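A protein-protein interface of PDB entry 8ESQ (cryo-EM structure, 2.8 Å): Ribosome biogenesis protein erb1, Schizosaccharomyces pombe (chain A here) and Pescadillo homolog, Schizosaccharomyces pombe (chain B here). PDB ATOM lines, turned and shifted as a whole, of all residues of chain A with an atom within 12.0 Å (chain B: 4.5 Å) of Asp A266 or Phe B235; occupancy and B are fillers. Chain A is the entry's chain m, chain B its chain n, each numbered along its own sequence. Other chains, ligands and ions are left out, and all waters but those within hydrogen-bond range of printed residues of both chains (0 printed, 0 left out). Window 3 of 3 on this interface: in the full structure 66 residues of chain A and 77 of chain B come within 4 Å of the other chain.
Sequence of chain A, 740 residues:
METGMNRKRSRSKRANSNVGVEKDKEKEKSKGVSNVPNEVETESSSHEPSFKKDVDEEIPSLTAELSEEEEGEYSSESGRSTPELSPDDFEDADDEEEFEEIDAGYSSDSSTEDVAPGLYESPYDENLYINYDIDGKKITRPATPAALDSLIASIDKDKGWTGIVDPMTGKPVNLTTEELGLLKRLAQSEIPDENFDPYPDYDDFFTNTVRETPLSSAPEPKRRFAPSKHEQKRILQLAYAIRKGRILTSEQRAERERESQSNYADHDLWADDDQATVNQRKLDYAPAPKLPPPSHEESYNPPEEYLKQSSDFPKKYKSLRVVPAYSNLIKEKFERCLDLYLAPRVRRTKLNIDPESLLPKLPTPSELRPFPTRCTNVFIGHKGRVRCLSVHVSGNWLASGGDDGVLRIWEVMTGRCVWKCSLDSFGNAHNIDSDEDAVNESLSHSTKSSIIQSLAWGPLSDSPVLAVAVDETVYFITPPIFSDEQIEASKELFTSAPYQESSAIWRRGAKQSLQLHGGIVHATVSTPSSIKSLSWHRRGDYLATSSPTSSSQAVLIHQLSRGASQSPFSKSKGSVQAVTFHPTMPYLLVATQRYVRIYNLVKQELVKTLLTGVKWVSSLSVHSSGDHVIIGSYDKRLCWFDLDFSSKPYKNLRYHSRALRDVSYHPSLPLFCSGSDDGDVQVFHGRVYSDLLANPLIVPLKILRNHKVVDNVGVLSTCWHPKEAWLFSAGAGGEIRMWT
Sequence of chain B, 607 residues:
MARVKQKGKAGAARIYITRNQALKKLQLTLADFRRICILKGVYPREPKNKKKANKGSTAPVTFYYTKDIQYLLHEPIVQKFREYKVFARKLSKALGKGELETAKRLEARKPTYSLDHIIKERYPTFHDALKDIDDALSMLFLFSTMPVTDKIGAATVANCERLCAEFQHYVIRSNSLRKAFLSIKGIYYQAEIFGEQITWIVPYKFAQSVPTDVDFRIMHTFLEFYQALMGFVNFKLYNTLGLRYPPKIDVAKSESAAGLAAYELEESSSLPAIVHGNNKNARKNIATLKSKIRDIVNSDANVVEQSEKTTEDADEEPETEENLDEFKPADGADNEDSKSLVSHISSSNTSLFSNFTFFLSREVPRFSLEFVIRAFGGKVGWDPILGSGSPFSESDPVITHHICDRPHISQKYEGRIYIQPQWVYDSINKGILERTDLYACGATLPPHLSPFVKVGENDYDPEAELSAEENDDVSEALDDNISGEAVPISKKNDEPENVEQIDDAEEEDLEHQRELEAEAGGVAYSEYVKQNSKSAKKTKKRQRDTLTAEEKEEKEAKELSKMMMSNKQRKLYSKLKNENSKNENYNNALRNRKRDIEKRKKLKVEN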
ATOM      1  N   GLU A 259     -18.911   8.730 -38.206  1.00  0.00           N
ATOM      2  CA  GLU A 259     -19.326   9.591 -37.102  1.00  0.00           C
ATOM      3  C   GLU A 259     -18.595   9.246 -35.812  1.00  0.00           C
ATOM      4  O   GLU A 259     -18.368  10.126 -34.974  1.00  0.00           O
ATOM      5  CB  GLU A 259     -20.838   9.501 -36.896  1.00  0.00           C
ATOM      6  CG  GLU A 259     -21.658   9.889 -38.117  1.00  0.00           C
ATOM      7  CD  GLU A 259     -22.924   9.066 -38.257  1.00  0.00           C
ATOM      8  OE1 GLU A 259     -23.382   8.499 -37.242  1.00  0.00           O
ATOM      9  OE2 GLU A 259     -23.457   8.981 -39.384  1.00  0.00           O
ATOM     10  N   SER A 260     -18.219   7.983 -35.631  1.00  0.00           N
ATOM     11  CA  SER A 260     -17.470   7.567 -34.453  1.00  0.00           C
ATOM     12  C   SER A 260     -15.993   7.913 -34.643  1.00  0.00           C
ATOM     13  O   SER A 260     -15.616   8.657 -35.553  1.00  0.00           O
ATOM     14  CB  SER A 260     -17.678   6.081 -34.184  1.00  0.00           C
ATOM     15  OG  SER A 260     -16.744   5.606 -33.229  1.00  0.00           O
ATOM     16  N   GLN A 261     -15.141   7.367 -33.773  1.00  0.00           N
ATOM     17  CA  GLN A 261     -13.710   7.672 -33.765  1.00  0.00           C
ATOM     18  C   GLN A 261     -13.470   9.170 -33.601  1.00  0.00           C
ATOM     19  O   GLN A 261     -12.589   9.753 -34.236  1.00  0.00           O
ATOM     20  CB  GLN A 261     -13.018   7.142 -35.025  1.00  0.00           C
ATOM     21  CG  GLN A 261     -12.737   5.647 -35.012  1.00  0.00           C
ATOM     22  CD  GLN A 261     -11.659   5.254 -34.018  1.00  0.00           C
ATOM     23  OE1 GLN A 261     -10.928   6.103 -33.508  1.00  0.00           O
ATOM     24  NE2 GLN A 261     -11.551   3.959 -33.744  1.00  0.00           N
ATOM     25  N   SER A 262     -14.264   9.800 -32.734  1.00  0.00           N
ATOM     26  CA  SER A 262     -14.180  11.240 -32.493  1.00  0.00           C
ATOM     27  C   SER A 262     -14.412  11.478 -31.004  1.00  0.00           C
ATOM     28  O   SER A 262     -15.558  11.542 -30.551  1.00  0.00           O
ATOM     29  CB  SER A 262     -15.189  12.003 -33.343  1.00  0.00           C
ATOM     30  OG  SER A 262     -14.973  11.770 -34.722  1.00  0.00           O
ATOM     31  N   ASN A 263     -13.322  11.610 -30.251  1.00  0.00           N
ATOM     32  CA  ASN A 263     -13.410  11.864 -28.815  1.00  0.00           C
ATOM     33  C   ASN A 263     -12.141  12.589 -28.387  1.00  0.00           C
ATOM     34  O   ASN A 263     -11.051  12.013 -28.442  1.00  0.00           O
ATOM     35  CB  ASN A 263     -13.602  10.561 -28.042  1.00  0.00           C
ATOM     36  CG  ASN A 263     -12.701   9.441 -28.539  1.00  0.00           C
ATOM     37  OD1 ASN A 263     -11.852   9.643 -29.409  1.00  0.00           O
ATOM     38  ND2 ASN A 263     -12.888   8.247 -27.988  1.00  0.00           N
ATOM     39  N   TYR A 264     -12.281  13.848 -27.969  1.00  0.00           N
ATOM     40  CA  TYR A 264     -11.110  14.640 -27.589  1.00  0.00           C
ATOM     41  C   TYR A 264     -11.524  15.600 -26.474  1.00  0.00           C
ATOM     42  O   TYR A 264     -11.967  16.719 -26.741  1.00  0.00           O
ATOM     43  CB  TYR A 264     -10.549  15.388 -28.788  1.00  0.00           C
ATOM     44  CG  TYR A 264      -9.765  14.514 -29.737  1.00  0.00           C
ATOM     45  CD1 TYR A 264      -8.503  14.045 -29.399  1.00  0.00           C
ATOM     46  CD2 TYR A 264     -10.292  14.152 -30.971  1.00  0.00           C
ATOM     47  CE1 TYR A 264      -7.785  13.244 -30.265  1.00  0.00           C
ATOM     48  CE2 TYR A 264      -9.582  13.350 -31.843  1.00  0.00           C
ATOM     49  CZ  TYR A 264      -8.329  12.901 -31.485  1.00  0.00           C
ATOM     50  OH  TYR A 264      -7.617  12.103 -32.350  1.00  0.00           O
ATOM     51  N   ALA A 265     -11.347  15.153 -25.230  1.00  0.00           N
ATOM     52  CA  ALA A 265     -11.507  15.981 -24.034  1.00  0.00           C
ATOM     53  C   ALA A 265     -12.803  16.794 -24.080  1.00  0.00           C
ATOM     54  O   ALA A 265     -12.805  18.022 -24.136  1.00  0.00           O
ATOM     55  CB  ALA A 265     -10.292  16.894 -23.857  1.00  0.00           C
ATOM     56  N   ASP A 266     -13.916  16.068 -24.065  1.00  0.00           N
ATOM     57  CA  ASP A 266     -15.224  16.673 -24.272  1.00  0.00           C
ATOM     58  C   ASP A 266     -15.929  17.078 -22.983  1.00  0.00           C
ATOM     59  O   ASP A 266     -17.028  17.638 -23.054  1.00  0.00           O
ATOM     60  CB  ASP A 266     -16.121  15.716 -25.062  1.00  0.00           C
ATOM     61  CG  ASP A 266     -16.157  14.326 -24.463  1.00  0.00           C
ATOM     62  OD1 ASP A 266     -15.295  13.497 -24.826  1.00  0.00           O
ATOM     63  OD2 ASP A 266     -17.047  14.059 -23.628  1.00  0.00           O
ATOM     64  N   HIS A 267     -15.345  16.827 -21.814  1.00  0.00           N
ATOM     65  CA  HIS A 267     -16.013  17.161 -20.566  1.00  0.00           C
ATOM     66  C   HIS A 267     -15.000  17.689 -19.561  1.00  0.00           C
ATOM     67  O   HIS A 267     -13.791  17.492 -19.699  1.00  0.00           O
ATOM     68  CB  HIS A 267     -16.766  15.958 -19.980  1.00  0.00           C
ATOM     69  CG  HIS A 267     -15.919  15.063 -19.132  1.00  0.00           C
ATOM     70  ND1 HIS A 267     -15.161  14.038 -19.657  1.00  0.00           N
ATOM     71  CD2 HIS A 267     -15.725  15.024 -17.793  1.00  0.00           C
ATOM     72  CE1 HIS A 267     -14.529  13.416 -18.678  1.00  0.00           C
ATOM     73  NE2 HIS A 267     -14.855  13.994 -17.538  1.00  0.00           N
ATOM     74  N   ASP A 268     -15.518  18.378 -18.550  1.00  0.00           N
ATOM     75  CA  ASP A 268     -14.708  19.037 -17.531  1.00  0.00           C
ATOM     76  C   ASP A 268     -14.600  18.120 -16.316  1.00  0.00           C
ATOM     77  O   ASP A 268     -15.578  17.931 -15.587  1.00  0.00           O
ATOM     78  CB  ASP A 268     -15.330  20.379 -17.151  1.00  0.00           C
ATOM     79  CG  ASP A 268     -14.463  21.179 -16.207  1.00  0.00           C
ATOM     80  OD1 ASP A 268     -13.289  20.806 -16.017  1.00  0.00           O
ATOM     81  OD2 ASP A 268     -14.957  22.179 -15.649  1.00  0.00           O
ATOM     82  N   LEU A 269     -13.410  17.552 -16.097  1.00  0.00           N
ATOM     83  CA  LEU A 269     -13.207  16.723 -14.913  1.00  0.00           C
ATOM     84  C   LEU A 269     -13.343  17.535 -13.637  1.00  0.00           C
ATOM     85  O   LEU A 269     -13.660  16.983 -12.577  1.00  0.00           O
ATOM     86  CB  LEU A 269     -11.829  16.066 -14.941  1.00  0.00           C
ATOM     87  CG  LEU A 269     -11.363  15.313 -16.179  1.00  0.00           C
ATOM     88  CD1 LEU A 269      -9.874  15.497 -16.299  1.00  0.00           C
ATOM     89  CD2 LEU A 269     -11.715  13.844 -16.073  1.00  0.00           C
ATOM     90  N   TRP A 270     -13.115  18.839 -13.721  1.00  0.00           N
ATOM     91  CA  TRP A 270     -12.994  19.704 -12.559  1.00  0.00           C
ATOM     92  C   TRP A 270     -14.332  20.243 -12.076  1.00  0.00           C
ATOM     93  O   TRP A 270     -14.353  21.041 -11.133  1.00  0.00           O
ATOM     94  CB  TRP A 270     -12.046  20.855 -12.892  1.00  0.00           C
ATOM     95  CG  TRP A 270     -10.839  20.380 -13.638  1.00  0.00           C
ATOM     96  CD1 TRP A 270     -10.556  20.578 -14.956  1.00  0.00           C
ATOM     97  CD2 TRP A 270      -9.760  19.607 -13.110  1.00  0.00           C
ATOM     98  NE1 TRP A 270      -9.363  19.985 -15.281  1.00  0.00           N
ATOM     99  CE2 TRP A 270      -8.852  19.382 -14.163  1.00  0.00           C
ATOM    100  CE3 TRP A 270      -9.468  19.090 -11.848  1.00  0.00           C
ATOM    101  CZ2 TRP A 270      -7.679  18.662 -13.992  1.00  0.00           C
ATOM    102  CZ3 TRP A 270      -8.307  18.380 -11.682  1.00  0.00           C
ATOM    103  CH2 TRP A 270      -7.425  18.168 -12.745  1.00  0.00           C
ATOM    104  N   ALA A 271     -15.434  19.832 -12.699  1.00  0.00           N
ATOM    105  CA  ALA A 271     -16.780  20.222 -12.286  1.00  0.00           C
ATOM    106  C   ALA A 271     -16.952  21.735 -12.254  1.00  0.00           C
ATOM    107  O   ALA A 271     -17.464  22.287 -11.281  1.00  0.00           O
ATOM    108  CB  ALA A 271     -17.112  19.623 -10.925  1.00  0.00           C
ATOM    109  N   GLY B 231      -5.273  18.153 -22.780  1.00  0.00           N
ATOM    110  CA  GLY B 231      -6.580  18.198 -23.413  1.00  0.00           C
ATOM    111  C   GLY B 231      -7.675  18.584 -22.441  1.00  0.00           C
ATOM    112  O   GLY B 231      -8.576  19.357 -22.771  1.00  0.00           O
ATOM    113  N   PHE B 232      -7.615  18.041 -21.225  1.00  0.00           N
ATOM    114  CA  PHE B 232      -8.618  18.373 -20.219  1.00  0.00           C
ATOM    115  C   PHE B 232      -8.375  19.754 -19.628  1.00  0.00           C
ATOM    116  O   PHE B 232      -9.326  20.483 -19.325  1.00  0.00           O
ATOM    117  CB  PHE B 232      -8.627  17.301 -19.132  1.00  0.00           C
ATOM    118  CG  PHE B 232      -9.097  15.965 -19.619  1.00  0.00           C
ATOM    119  CD1 PHE B 232     -10.226  15.864 -20.409  1.00  0.00           C
ATOM    120  CD2 PHE B 232      -8.399  14.811 -19.308  1.00  0.00           C
ATOM    121  CE1 PHE B 232     -10.658  14.640 -20.869  1.00  0.00           C
ATOM    122  CE2 PHE B 232      -8.827  13.582 -19.764  1.00  0.00           C
ATOM    123  CZ  PHE B 232      -9.956  13.499 -20.549  1.00  0.00           C
ATOM    124  N   VAL B 233      -7.107  20.130 -19.449  1.00  0.00           N
ATOM    125  CA  VAL B 233      -6.787  21.462 -18.946  1.00  0.00           C
ATOM    126  C   VAL B 233      -7.209  22.529 -19.947  1.00  0.00           C
ATOM    127  O   VAL B 233      -7.828  23.534 -19.581  1.00  0.00           O
ATOM    128  CB  VAL B 233      -5.287  21.558 -18.614  1.00  0.00           C
ATOM    129  CG1 VAL B 233      -4.860  23.006 -18.497  1.00  0.00           C
ATOM    130  CG2 VAL B 233      -4.984  20.811 -17.329  1.00  0.00           C
ATOM    131  N   ASN B 234      -6.889  22.326 -21.227  1.00  0.00           N
ATOM    132  CA  ASN B 234      -7.255  23.306 -22.244  1.00  0.00           C
ATOM    133  C   ASN B 234      -8.765  23.394 -22.408  1.00  0.00           C
ATOM    134  O   ASN B 234      -9.303  24.464 -22.712  1.00  0.00           O
ATOM    135  CB  ASN B 234      -6.593  22.961 -23.575  1.00  0.00           C
ATOM    136  CG  ASN B 234      -5.108  23.242 -23.575  1.00  0.00           C
ATOM    137  OD1 ASN B 234      -4.639  24.153 -22.897  1.00  0.00           O
ATOM    138  ND2 ASN B 234      -4.358  22.463 -24.342  1.00  0.00           N
ATOM    139  N   PHE B 235      -9.465  22.274 -22.228  1.00  0.00           N
ATOM    140  CA  PHE B 235     -10.919  22.284 -22.346  1.00  0.00           C
ATOM    141  C   PHE B 235     -11.549  23.181 -21.289  1.00  0.00           C
ATOM    142  O   PHE B 235     -12.473  23.950 -21.581  1.00  0.00           O
ATOM    143  CB  PHE B 235     -11.461  20.862 -22.237  1.00  0.00           C
ATOM    144  CG  PHE B 235     -12.958  20.780 -22.277  1.00  0.00           C
ATOM    145  CD1 PHE B 235     -13.633  20.866 -23.480  1.00  0.00           C
ATOM    146  CD2 PHE B 235     -13.687  20.609 -21.115  1.00  0.00           C
ATOM    147  CE1 PHE B 235     -15.009  20.786 -23.526  1.00  0.00           C
ATOM    148  CE2 PHE B 235     -15.063  20.527 -21.155  1.00  0.00           C
ATOM    149  CZ  PHE B 235     -15.725  20.614 -22.362  1.00  0.00           C
ATOM    150  N   LYS B 236     -11.069  23.092 -20.046  1.00  0.00           N
ATOM    151  CA  LYS B 236     -11.604  23.948 -18.994  1.00  0.00           C
ATOM    152  C   LYS B 236     -11.215  25.403 -19.214  1.00  0.00           C
ATOM    153  O   LYS B 236     -12.032  26.309 -19.012  1.00  0.00           O
ATOM    154  CB  LYS B 236     -11.127  23.474 -17.623  1.00  0.00           C
ATOM    155  CG  LYS B 236     -11.704  24.291 -16.480  1.00  0.00           C
ATOM    156  CD  LYS B 236     -11.169  23.844 -15.137  1.00  0.00           C
ATOM    157  CE  LYS B 236     -11.858  24.580 -14.000  1.00  0.00           C
ATOM    158  NZ  LYS B 236     -13.303  24.236 -13.914  1.00  0.00           N
ATOM    159  N   LEU B 237      -9.969  25.646 -19.622  1.00  0.00           N
ATOM    160  CA  LEU B 237      -9.512  27.016 -19.832  1.00  0.00           C
ATOM    161  C   LEU B 237     -10.330  27.711 -20.912  1.00  0.00           C
ATOM    162  O   LEU B 237     -10.688  28.886 -20.772  1.00  0.00           O
ATOM    163  CB  LEU B 237      -8.029  27.023 -20.195  1.00  0.00           C
ATOM    164  CG  LEU B 237      -7.059  26.705 -19.058  1.00  0.00           C
ATOM    165  CD1 LEU B 237      -5.623  26.775 -19.542  1.00  0.00           C
ATOM    166  CD2 LEU B 237      -7.279  27.651 -17.896  1.00  0.00           C
ATOM    167  N   TYR B 238     -10.633  27.002 -21.999  1.00  0.00           N
ATOM    168  CA  TYR B 238     -11.456  27.586 -23.052  1.00  0.00           C
ATOM    169  C   TYR B 238     -12.883  27.821 -22.572  1.00  0.00           C
ATOM    170  O   TYR B 238     -13.501  28.835 -22.911  1.00  0.00           O
ATOM    171  CB  TYR B 238     -11.438  26.687 -24.286  1.00  0.00           C
ATOM    172  CG  TYR B 238     -10.253  26.935 -25.191  1.00  0.00           C
ATOM    173  CD1 TYR B 238      -8.970  27.032 -24.675  1.00  0.00           C
ATOM    174  CD2 TYR B 238     -10.420  27.077 -26.558  1.00  0.00           C
ATOM    175  CE1 TYR B 238      -7.887  27.261 -25.494  1.00  0.00           C
ATOM    176  CE2 TYR B 238      -9.343  27.306 -27.385  1.00  0.00           C
ATOM    177  CZ  TYR B 238      -8.080  27.399 -26.848  1.00  0.00           C
ATOM    178  OH  TYR B 238      -7.004  27.628 -27.672  1.00  0.00           O
ATOM    179  N   ASN B 239     -13.426  26.889 -21.785  1.00  0.00           N
ATOM    180  CA  ASN B 239     -14.775  27.064 -21.256  1.00  0.00           C
ATOM    181  C   ASN B 239     -14.836  28.208 -20.254  1.00  0.00           C
ATOM    182  O   ASN B 239     -15.824  28.952 -20.210  1.00  0.00           O
ATOM    183  CB  ASN B 239     -15.258  25.767 -20.616  1.00  0.00           C
ATOM    184  CG  ASN B 239     -15.622  24.724 -21.639  1.00  0.00           C
ATOM    185  OD1 ASN B 239     -16.403  24.979 -22.554  1.00  0.00           O
ATOM    186  ND2 ASN B 239     -15.037  23.547 -21.508  1.00  0.00           N
ATOM    187  N   TYR B 245     -14.344  24.298 -27.198  1.00  0.00           N
ATOM    188  CA  TYR B 245     -13.208  23.405 -27.334  1.00  0.00           C
ATOM    189  C   TYR B 245     -13.622  22.127 -28.047  1.00  0.00           C
ATOM    190  O   TYR B 245     -14.662  21.539 -27.724  1.00  0.00           O
ATOM    191  CB  TYR B 245     -12.609  23.057 -25.968  1.00  0.00           C
ATOM    192  CG  TYR B 245     -11.195  22.538 -26.044  1.00  0.00           C
ATOM    193  CD1 TYR B 245     -10.128  23.403 -26.221  1.00  0.00           C
ATOM    194  CD2 TYR B 245     -10.927  21.180 -25.941  1.00  0.00           C
ATOM    195  CE1 TYR B 245      -8.835  22.935 -26.292  1.00  0.00           C
ATOM    196  CE2 TYR B 245      -9.635  20.702 -26.010  1.00  0.00           C
ATOM    197  CZ  TYR B 245      -8.593  21.584 -26.185  1.00  0.00           C
ATOM    198  OH  TYR B 245      -7.303  21.117 -26.256  1.00  0.00           O
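Among the printed residues, pairs that only touch across the chains: Ala A265 with Phe B235 (3.0 Å), Ala A265 with Gly B231 (3.2 Å), His A267 with Phe B235 (3.3 Å), Asp A266 with Phe B235 (3.3 Å), Trp A270 with Lys B236 (3.3 Å), Asp A268 with Phe B235 (3.4 Å), Leu A269 with Phe B232 (3.4 Å), Ala A265 with Phe B232 (3.5 Å) and His A267 with Phe B232 (3.98 Å).
The side-chain carboxylate of Asp A268 is in salt-bridge range of the side-chain amino group of Lys B236, at 3.2 Å.
The side-chain carboxylate (OD1) of Asp A268 lies close to the backbone NH (N) of Trp A270, at 3.0 Å. The backbone carbonyl oxygen (O) of Phe B235 sits at hydrogen-bond distance from the side-chain amide nitrogen (ND2) of Asn B239, 2.6 Å away.
Hydrophobic or aromatic side chains of chain A within 4 Å of the printed part of chain B: Ala A265, Leu A269 and Trp A270. Among the printed residues, 10 pairs touch across the chains. Among the printed residues, Asp or Glu carboxylates within 4 Å of a Lys or Arg side-chain nitrogen of the other chain: Asp A268 with Lys B236 (3.2 Å).
Asp A266 touches just one residue of chain B: Phe B235 (3.3 Å). Phe B235 touches just these residues of chain A: Ala A265 (3.0 Å), Asp A266 (3.3 Å), His A267 (3.3 Å) and Asp A268 (3.4 Å). Of the printed residues of chain A, Gly B231 touches Ala A265. No residue of chain A comes within 4 Å of Asn B234. Lys B236 touches just these residues of chain A: Asp A268 and Trp A270. No residue of chain A comes within 4 Å of Leu B237. No residue of chain A comes within 4 Å of Asn B239. No residue of chain A comes within 4 Å of Tyr B245. Printed residues of chain A within 4 Å of Phe B232: Ala A265, His A267 and Leu A269. Of the printed residues of chain B, Asp A268 touches Phe B235 and Lys B236. Of the printed residues of chain B, His A267 touches Phe B232 and Phe B235. The nearest residue of chain A that does not touch Phe B235 is Tyr A264 (5.5 Å). The nearest printed residue of chain B that does not touch Ala A265 is Tyr B245 (4.1 Å).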
